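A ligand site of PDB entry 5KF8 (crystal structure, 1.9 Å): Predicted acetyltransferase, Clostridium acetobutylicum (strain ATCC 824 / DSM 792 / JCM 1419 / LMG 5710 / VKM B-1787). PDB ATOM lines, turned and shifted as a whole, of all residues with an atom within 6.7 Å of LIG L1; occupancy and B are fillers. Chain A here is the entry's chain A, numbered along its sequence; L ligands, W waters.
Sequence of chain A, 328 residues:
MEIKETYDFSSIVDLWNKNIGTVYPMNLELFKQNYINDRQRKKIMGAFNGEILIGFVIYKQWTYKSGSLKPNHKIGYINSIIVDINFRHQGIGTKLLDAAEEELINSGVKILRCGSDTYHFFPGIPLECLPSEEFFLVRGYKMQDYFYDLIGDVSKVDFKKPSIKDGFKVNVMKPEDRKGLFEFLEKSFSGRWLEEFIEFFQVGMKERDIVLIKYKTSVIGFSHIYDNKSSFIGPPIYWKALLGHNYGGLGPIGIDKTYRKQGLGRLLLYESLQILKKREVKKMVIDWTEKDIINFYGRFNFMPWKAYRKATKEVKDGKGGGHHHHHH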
ATOM      1  N   HIS A 120       8.787   1.384  25.866  1.00  0.00           N
ATOM      2  CA  HIS A 120       8.306   0.905  27.158  1.00  0.00           C
ATOM      3  C   HIS A 120       7.772   2.049  27.996  1.00  0.00           C
ATOM      4  O   HIS A 120       8.119   3.223  27.799  1.00  0.00           O
ATOM      5  CB  HIS A 120       9.474   0.270  27.936  1.00  0.00           C
ATOM      6  CG  HIS A 120      10.587   1.211  28.241  1.00  0.00           C
ATOM      7  ND1 HIS A 120      11.420   1.738  27.273  1.00  0.00           N
ATOM      8  CD2 HIS A 120      11.026   1.689  29.432  1.00  0.00           C
ATOM      9  CE1 HIS A 120      12.304   2.535  27.850  1.00  0.00           C
ATOM     10  NE2 HIS A 120      12.088   2.509  29.160  1.00  0.00           N
ATOM     11  N   ARG A 192      19.710  -1.663  19.947  1.00  0.00           N
ATOM     12  CA  ARG A 192      18.591  -0.815  20.333  1.00  0.00           C
ATOM     13  C   ARG A 192      18.927   0.707  20.281  1.00  0.00           C
ATOM     14  O   ARG A 192      18.062   1.525  19.937  1.00  0.00           O
ATOM     15  CB  ARG A 192      18.156  -1.192  21.780  1.00  0.00           C
ATOM     16  CG  ARG A 192      17.097  -0.271  22.302  1.00  0.00           C
ATOM     17  CD  ARG A 192      16.331  -0.854  23.488  1.00  0.00           C
ATOM     18  NE  ARG A 192      15.303   0.079  23.923  1.00  0.00           N
ATOM     19  CZ  ARG A 192      14.216  -0.278  24.616  1.00  0.00           C
ATOM     20  NH1 ARG A 192      13.323   0.635  24.974  1.00  0.00           N
ATOM     21  NH2 ARG A 192      13.976  -1.564  24.873  1.00  0.00           N
ATOM     22  N   TRP A 193      20.145   1.079  20.636  1.00  0.00           N
ATOM     23  CA  TRP A 193      20.482   2.488  20.717  1.00  0.00           C
ATOM     24  C   TRP A 193      20.575   3.093  19.318  1.00  0.00           C
ATOM     25  O   TRP A 193      20.147   4.239  19.098  1.00  0.00           O
ATOM     26  CB  TRP A 193      21.791   2.656  21.510  1.00  0.00           C
ATOM     27  CG  TRP A 193      21.642   2.486  23.016  1.00  0.00           C
ATOM     28  CD1 TRP A 193      20.498   2.213  23.695  1.00  0.00           C
ATOM     29  CD2 TRP A 193      22.665   2.598  24.013  1.00  0.00           C
ATOM     30  NE1 TRP A 193      20.733   2.120  25.037  1.00  0.00           N
ATOM     31  CE2 TRP A 193      22.049   2.376  25.274  1.00  0.00           C
ATOM     32  CE3 TRP A 193      24.052   2.872  23.978  1.00  0.00           C
ATOM     33  CZ2 TRP A 193      22.767   2.405  26.488  1.00  0.00           C
ATOM     34  CZ3 TRP A 193      24.767   2.898  25.183  1.00  0.00           C
ATOM     35  CH2 TRP A 193      24.116   2.660  26.425  1.00  0.00           C
ATOM     36  N   GLU A 196      16.986   3.531  18.379  1.00  0.00           N
ATOM     37  CA  GLU A 196      16.411   4.684  19.057  1.00  0.00           C
ATOM     38  C   GLU A 196      16.822   5.983  18.340  1.00  0.00           C
ATOM     39  O   GLU A 196      16.022   6.902  18.177  1.00  0.00           O
ATOM     40  CB  GLU A 196      16.825   4.776  20.538  1.00  0.00           C
ATOM     41  CG  GLU A 196      16.224   3.657  21.396  1.00  0.00           C
ATOM     42  CD  GLU A 196      16.706   3.698  22.859  1.00  0.00           C
ATOM     43  OE1 GLU A 196      17.516   4.582  23.234  1.00  0.00           O
ATOM     44  OE2 GLU A 196      16.218   2.837  23.601  1.00  0.00           O
ATOM     45  N   PHE A 200      13.927   8.253  17.214  1.00  0.00           N
ATOM     46  CA  PHE A 200      13.784   9.485  17.949  1.00  0.00           C
ATOM     47  C   PHE A 200      13.983  10.707  17.014  1.00  0.00           C
ATOM     48  O   PHE A 200      13.263  11.727  17.156  1.00  0.00           O
ATOM     49  CB  PHE A 200      14.769   9.550  19.129  1.00  0.00           C
ATOM     50  CG  PHE A 200      14.515   8.532  20.224  1.00  0.00           C
ATOM     51  CD1 PHE A 200      13.457   7.630  20.161  1.00  0.00           C
ATOM     52  CD2 PHE A 200      15.367   8.482  21.332  1.00  0.00           C
ATOM     53  CE1 PHE A 200      13.229   6.697  21.165  1.00  0.00           C
ATOM     54  CE2 PHE A 200      15.137   7.572  22.352  1.00  0.00           C
ATOM     55  CZ  PHE A 200      14.070   6.664  22.261  1.00  0.00           C
ATOM     56  N   PRO A 235      12.669   8.329  27.871  1.00  0.00           N
ATOM     57  CA  PRO A 235      12.542   7.676  29.164  1.00  0.00           C
ATOM     58  C   PRO A 235      13.024   8.478  30.382  1.00  0.00           C
ATOM     59  O   PRO A 235      12.340   8.493  31.414  1.00  0.00           O
ATOM     60  CB  PRO A 235      13.377   6.392  28.965  1.00  0.00           C
ATOM     61  CG  PRO A 235      13.331   6.084  27.544  1.00  0.00           C
ATOM     62  CD  PRO A 235      13.255   7.422  26.854  1.00  0.00           C
ATOM     63  N   PRO A 236      14.151   9.203  30.285  1.00  0.00           N
ATOM     64  CA  PRO A 236      14.523  10.042  31.453  1.00  0.00           C
ATOM     65  C   PRO A 236      13.462  11.002  31.945  1.00  0.00           C
ATOM     66  O   PRO A 236      13.458  11.412  33.121  1.00  0.00           O
ATOM     67  CB  PRO A 236      15.710  10.837  30.926  1.00  0.00           C
ATOM     68  CG  PRO A 236      16.342   9.926  29.907  1.00  0.00           C
ATOM     69  CD  PRO A 236      15.148   9.306  29.208  1.00  0.00           C
ATOM     70  N   LEU A 250      19.154  12.439  31.404  1.00  0.00           N
ATOM     71  CA  LEU A 250      20.233  11.969  30.609  1.00  0.00           C
ATOM     72  C   LEU A 250      20.165  10.449  30.421  1.00  0.00           C
ATOM     73  O   LEU A 250      20.026   9.685  31.369  1.00  0.00           O
ATOM     74  CB  LEU A 250      21.529  12.380  31.295  1.00  0.00           C
ATOM     75  CG  LEU A 250      22.824  12.149  30.519  1.00  0.00           C
ATOM     76  CD1 LEU A 250      23.894  13.162  30.927  1.00  0.00           C
ATOM     77  CD2 LEU A 250      23.317  10.743  30.791  1.00  0.00           C
ATOM     78  N   GLY A 251      20.286  10.012  29.174  1.00  0.00           N
ATOM     79  CA  GLY A 251      20.500   8.592  28.901  1.00  0.00           C
ATOM     80  C   GLY A 251      19.905   8.346  27.542  1.00  0.00           C
ATOM     81  O   GLY A 251      18.917   9.013  27.152  1.00  0.00           O
ATOM     82  N   PRO A 252      20.540   7.466  26.771  1.00  0.00           N
ATOM     83  CA  PRO A 252      21.748   6.729  27.113  1.00  0.00           C
ATOM     84  C   PRO A 252      23.072   7.500  26.926  1.00  0.00           C
ATOM     85  O   PRO A 252      23.071   8.674  26.521  1.00  0.00           O
ATOM     86  CB  PRO A 252      21.758   5.585  26.108  1.00  0.00           C
ATOM     87  CG  PRO A 252      20.878   6.010  24.974  1.00  0.00           C
ATOM     88  CD  PRO A 252      19.854   6.943  25.569  1.00  0.00           C
ATOM     89  N   ILE A 253      24.172   6.839  27.260  1.00  0.00           N
ATOM     90  CA  ILE A 253      25.541   7.382  27.189  1.00  0.00           C
ATOM     91  C   ILE A 253      26.474   6.181  26.909  1.00  0.00           C
ATOM     92  O   ILE A 253      26.292   5.095  27.475  1.00  0.00           O
ATOM     93  CB  ILE A 253      25.914   8.128  28.484  1.00  0.00           C
ATOM     94  CG1 ILE A 253      27.289   8.769  28.398  1.00  0.00           C
ATOM     95  CG2 ILE A 253      25.899   7.192  29.661  1.00  0.00           C
ATOM     96  CD1 ILE A 253      27.588   9.695  29.545  1.00  0.00           C
ATOM     97  N   ILE A 286      18.385   9.880  35.430  1.00  0.00           N
ATOM     98  CA  ILE A 286      19.131   8.951  34.607  1.00  0.00           C
ATOM     99  C   ILE A 286      18.420   7.595  34.656  1.00  0.00           C
ATOM    100  O   ILE A 286      18.329   6.983  35.725  1.00  0.00           O
ATOM    101  CB  ILE A 286      20.608   8.886  35.064  1.00  0.00           C
ATOM    102  CG1 ILE A 286      21.155  10.331  35.021  1.00  0.00           C
ATOM    103  CG2 ILE A 286      21.350   7.942  34.127  1.00  0.00           C
ATOM    104  CD1 ILE A 286      22.551  10.550  35.498  1.00  0.00           C
ATOM    105  N   ASP A 287      17.882   7.150  33.530  1.00  0.00           N
ATOM    106  CA  ASP A 287      16.898   6.072  33.561  1.00  0.00           C
ATOM    107  C   ASP A 287      17.579   4.712  33.329  1.00  0.00           C
ATOM    108  O   ASP A 287      18.596   4.632  32.642  1.00  0.00           O
ATOM    109  CB  ASP A 287      15.821   6.274  32.473  1.00  0.00           C
ATOM    110  CG  ASP A 287      16.365   6.081  31.054  1.00  0.00           C
ATOM    111  OD1 ASP A 287      17.246   6.869  30.662  1.00  0.00           O
ATOM    112  OD2 ASP A 287      16.030   5.068  30.387  1.00  0.00           O
ATOM    113  N   TRP A 288      16.961   3.641  33.828  1.00  0.00           N
ATOM    114  CA  TRP A 288      17.325   2.249  33.472  1.00  0.00           C
ATOM    115  C   TRP A 288      18.852   1.985  33.459  1.00  0.00           C
ATOM    116  O   TRP A 288      19.486   1.698  32.399  1.00  0.00           O
ATOM    117  CB  TRP A 288      16.688   1.945  32.128  1.00  0.00           C
ATOM    118  CG  TRP A 288      16.581   0.470  31.728  1.00  0.00           C
ATOM    119  CD1 TRP A 288      17.189  -0.560  32.326  1.00  0.00           C
ATOM    120  CD2 TRP A 288      15.860  -0.090  30.608  1.00  0.00           C
ATOM    121  NE1 TRP A 288      16.919  -1.728  31.688  1.00  0.00           N
ATOM    122  CE2 TRP A 288      16.125  -1.468  30.599  1.00  0.00           C
ATOM    123  CE3 TRP A 288      15.025   0.445  29.606  1.00  0.00           C
ATOM    124  CZ2 TRP A 288      15.557  -2.356  29.672  1.00  0.00           C
ATOM    125  CZ3 TRP A 288      14.494  -0.409  28.659  1.00  0.00           C
ATOM    126  CH2 TRP A 288      14.757  -1.805  28.687  1.00  0.00           C
ATOM    127  N   THR A 289      19.395   2.052  34.662  1.00  0.00           N
ATOM    128  CA  THR A 289      20.773   1.696  35.003  1.00  0.00           C
ATOM    129  C   THR A 289      20.937   0.341  35.702  1.00  0.00           C
ATOM    130  O   THR A 289      20.079  -0.133  36.387  1.00  0.00           O
ATOM    131  CB  THR A 289      21.461   2.774  35.860  1.00  0.00           C
ATOM    132  OG1 THR A 289      20.912   2.870  37.207  1.00  0.00           O
ATOM    133  CG2 THR A 289      21.287   4.096  35.193  1.00  0.00           C
ATOM    134  N   GLU A 290      22.114  -0.262  35.551  1.00  0.00           N
ATOM    135  CA  GLU A 290      22.415  -1.495  36.277  1.00  0.00           C
ATOM    136  C   GLU A 290      23.084  -1.128  37.586  1.00  0.00           C
ATOM    137  O   GLU A 290      23.709  -0.063  37.728  1.00  0.00           O
ATOM    138  CB  GLU A 290      23.391  -2.352  35.476  1.00  0.00           C
ATOM    139  CG  GLU A 290      22.990  -2.552  34.049  1.00  0.00           C
ATOM    140  CD  GLU A 290      23.172  -3.972  33.603  1.00  0.00           C
ATOM    141  OE1 GLU A 290      24.160  -4.239  32.905  1.00  0.00           O
ATOM    142  OE2 GLU A 290      22.313  -4.799  33.956  1.00  0.00           O
ATOM    143  N   TYR A 297      27.575   7.403  38.086  1.00  0.00           N
ATOM    144  CA  TYR A 297      26.728   8.580  38.154  1.00  0.00           C
ATOM    145  C   TYR A 297      26.739   9.176  39.570  1.00  0.00           C
ATOM    146  O   TYR A 297      26.587  10.370  39.739  1.00  0.00           O
ATOM    147  CB  TYR A 297      25.297   8.183  37.750  1.00  0.00           C
ATOM    148  CG  TYR A 297      25.154   7.622  36.342  1.00  0.00           C
ATOM    149  CD1 TYR A 297      25.245   8.457  35.242  1.00  0.00           C
ATOM    150  CD2 TYR A 297      24.930   6.272  36.107  1.00  0.00           C
ATOM    151  CE1 TYR A 297      25.123   7.962  33.952  1.00  0.00           C
ATOM    152  CE2 TYR A 297      24.795   5.783  34.819  1.00  0.00           C
ATOM    153  CZ  TYR A 297      24.886   6.622  33.750  1.00  0.00           C
ATOM    154  OH  TYR A 297      24.710   6.149  32.460  1.00  0.00           O
HETATM  155  C1  LIG L   1      19.895   2.024  29.166  1.00  0.00           C
HETATM  156  C2  LIG L   1      20.101   3.513  29.363  1.00  0.00           C
HETATM  157  C3  LIG L   1      18.814   4.276  29.134  1.00  0.00           C
HETATM  158  C4  LIG L   1      17.980   3.833  27.913  1.00  0.00           C
HETATM  159  C5  LIG L   1      17.874   2.310  27.919  1.00  0.00           C
HETATM  160  C6  LIG L   1      17.202   1.619  26.720  1.00  0.00           C
HETATM  161  N1  LIG L   1      20.596   3.761  30.698  1.00  0.00           N
HETATM  162  O1  LIG L   1      21.113   1.279  29.229  1.00  0.00           O
HETATM  163  O2  LIG L   1      19.119   5.680  29.098  1.00  0.00           O
HETATM  164  O3  LIG L   1      16.674   4.405  27.874  1.00  0.00           O
HETATM  165  O4  LIG L   1      19.206   1.766  27.933  1.00  0.00           O
HETATM  166  O5  LIG L   1      17.873   1.930  25.476  1.00  0.00           O
HETATM  167  O1  LG2 L   2      22.503  -0.485  21.112  1.00  0.00           O
HETATM  168  S1  LG2 L   2      23.041  -1.633  21.770  1.00  0.00           S
HETATM  169  O2  LG2 L   2      21.932  -2.535  21.871  1.00  0.00           O
HETATM  170  O3  LG2 L   2      24.243  -2.348  20.954  1.00  0.00           O
HETATM  171  C1  LG2 L   2      23.764  -1.291  23.229  1.00  0.00           C
HETATM  172  C2  LG2 L   2      22.775  -1.640  24.308  1.00  0.00           C
HETATM  173  C3  LG2 L   2      23.411  -1.242  25.620  1.00  0.00           C
HETATM  174  N1  LG2 L   2      22.425  -1.283  26.722  1.00  0.00           N
HETATM  175  C4  LG2 L   2      21.040  -1.757  26.429  1.00  0.00           C
HETATM  176  C5  LG2 L   2      20.088  -1.527  27.607  1.00  0.00           C
HETATM  177  N2  LG2 L   2      20.717  -2.013  28.883  1.00  0.00           N
HETATM  178  C6  LG2 L   2      22.180  -1.825  29.059  1.00  0.00           C
HETATM  179  C7  LG2 L   2      23.052  -1.973  27.833  1.00  0.00           C
HETATM  180  C8  LG2 L   2      19.922  -1.644  30.067  1.00  0.00           C
HETATM  181  C9  LG2 L   2      20.650  -1.738  31.403  1.00  0.00           C
HETATM  182  O4  LG2 L   2      21.102  -0.443  31.776  1.00  0.00           O
HETATM  183  O1  LG3 L   3      35.417   7.258  31.790  1.00  0.00           O
HETATM  184  P1  LG3 L   3      35.451   6.188  32.856  1.00  0.00           P
HETATM  185  O2  LG3 L   3      35.084   6.528  34.284  1.00  0.00           O
HETATM  186  O3  LG3 L   3      36.909   5.519  32.852  1.00  0.00           O
HETATM  187  O4  LG3 L   3      34.502   4.976  32.375  1.00  0.00           O
HETATM  188  P2  LG3 L   3      34.438   4.549  30.827  1.00  0.00           P
HETATM  189  O5  LG3 L   3      35.460   5.370  30.064  1.00  0.00           O
HETATM  190  O6  LG3 L   3      34.471   3.049  30.744  1.00  0.00           O
HETATM  191  O7  LG3 L   3      32.973   5.043  30.383  1.00  0.00           O
HETATM  192  C1  LG3 L   3      30.744   4.152  30.117  1.00  0.00           C
HETATM  193  C2  LG3 L   3      31.822   4.609  31.102  1.00  0.00           C
HETATM  194  C3  LG3 L   3      29.560   3.570  30.881  1.00  0.00           C
HETATM  195  C4  LG3 L   3      30.292   5.332  29.266  1.00  0.00           C
HETATM  196  C5  LG3 L   3      31.332   3.075  29.215  1.00  0.00           C
HETATM  197  O8  LG3 L   3      31.789   1.976  30.002  1.00  0.00           O
HETATM  198  C6  LG3 L   3      30.279   2.609  28.256  1.00  0.00           C
HETATM  199  O9  LG3 L   3      30.004   3.258  27.265  1.00  0.00           O
HETATM  200  N1  LG3 L   3      29.681   1.457  28.555  1.00  0.00           N
HETATM  201  C7  LG3 L   3      28.795   0.800  27.624  1.00  0.00           C
HETATM  202  C8  LG3 L   3      27.438   1.506  27.515  1.00  0.00           C
HETATM  203  C9  LG3 L   3      26.798   1.569  28.886  1.00  0.00           C
HETATM  204  O10 LG3 L   3      26.586   0.545  29.521  1.00  0.00           O
HETATM  205  N2  LG3 L   3      26.499   2.782  29.339  1.00  0.00           N
HETATM  206  C10 LG3 L   3      25.794   2.967  30.594  1.00  0.00           C
HETATM  207  C11 LG3 L   3      24.286   2.946  30.423  1.00  0.00           C
HETATM  208  S1  LG3 L   3      23.490   3.298  32.007  1.00  0.00           S
HETATM  209  O   HOH W   1      16.215   5.821  25.495  1.00  0.00           O
HETATM  210  O   HOH W   2      22.064   6.264  30.946  1.00  0.00           O
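NE of Arg 192 lies within salt-bridge range of OE2 of Glu 196, at 2.9 Å.
NH1 of Arg 192 is in hydrogen-bond range of ND1 of His 120 (3.2 Å).
An oxygen (O1) of LIG L1 lies within hydrogen-bond range of an oxygen (O4) of LG2 L2, 3.1 Å away.
A nitrogen (N1) of LIG L1 sits close to a sulfur (S1) of LG3 L3 (3.2 Å).
OE2 of Glu 196 is in hydrogen-bond range of O5 of LIG L1 (2.7 Å).
The backbone carbonyl oxygen of Asp 287 is in hydrogen-bond range of a nitrogen (N1) of LIG L1 (2.9 Å).
O3 of LIG L1 lies within hydrogen-bond range of OD2 of Asp 287, 2.7 Å away.
The backbone carbonyl oxygen of Trp 288 lies within hydrogen-bond range of a nitrogen (N1) of LIG L1, 2.9 Å away.
NE1 of Trp 193 is in hydrogen-bond range of O5 of LIG L1.
O of Trp 288 sits at hydrogen-bond distance from O4 of LG2 L2 (2.8 Å).
O1 of LG2 L2 is in hydrogen-bond range of N of Trp 193.
N of Arg 192 lies within hydrogen-bond range of O2 of LG2 L2, 3.1 Å away.
The side-chain hydroxyl of Tyr 297 sits close to a sulfur (S1) of LG3 L3 (3.1 Å).
O of Ile 253 sits at hydrogen-bond distance from N2 of LG3 L3, 3.0 Å away.
The backbone nitrogen (N) of Pro 252 sits close to an oxygen (O2) of LIG L1 (3.3 Å).
Merely in contact with LIG L1: Gly 251 (3.2 Å), Arg 192 (3.5 Å) and Pro 235 (3.8 Å).
Hydrophobic or aromatic side chains that line LIG L1: Trp 193, Pro 235, Pro 252 and Trp 288.
Within 4 Å of LIG L1: Arg 192, Trp 193, Glu 196, Pro 235, Gly 251, Pro 252, Asp 287 and Trp 288.
The nearest printed residue that does not touch LIG L1 is Thr 289 (4.5 Å).
Water W1 lies within hydrogen-bond range of an oxygen (O3) of LIG L1 (2.8 Å) and the side-chain carboxylate (OE1) of Glu 196 (2.9 Å).
Water W2 lies within hydrogen-bond range of N1 of LIG L1, OH of Tyr 297 and S1 of LG3 L3.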
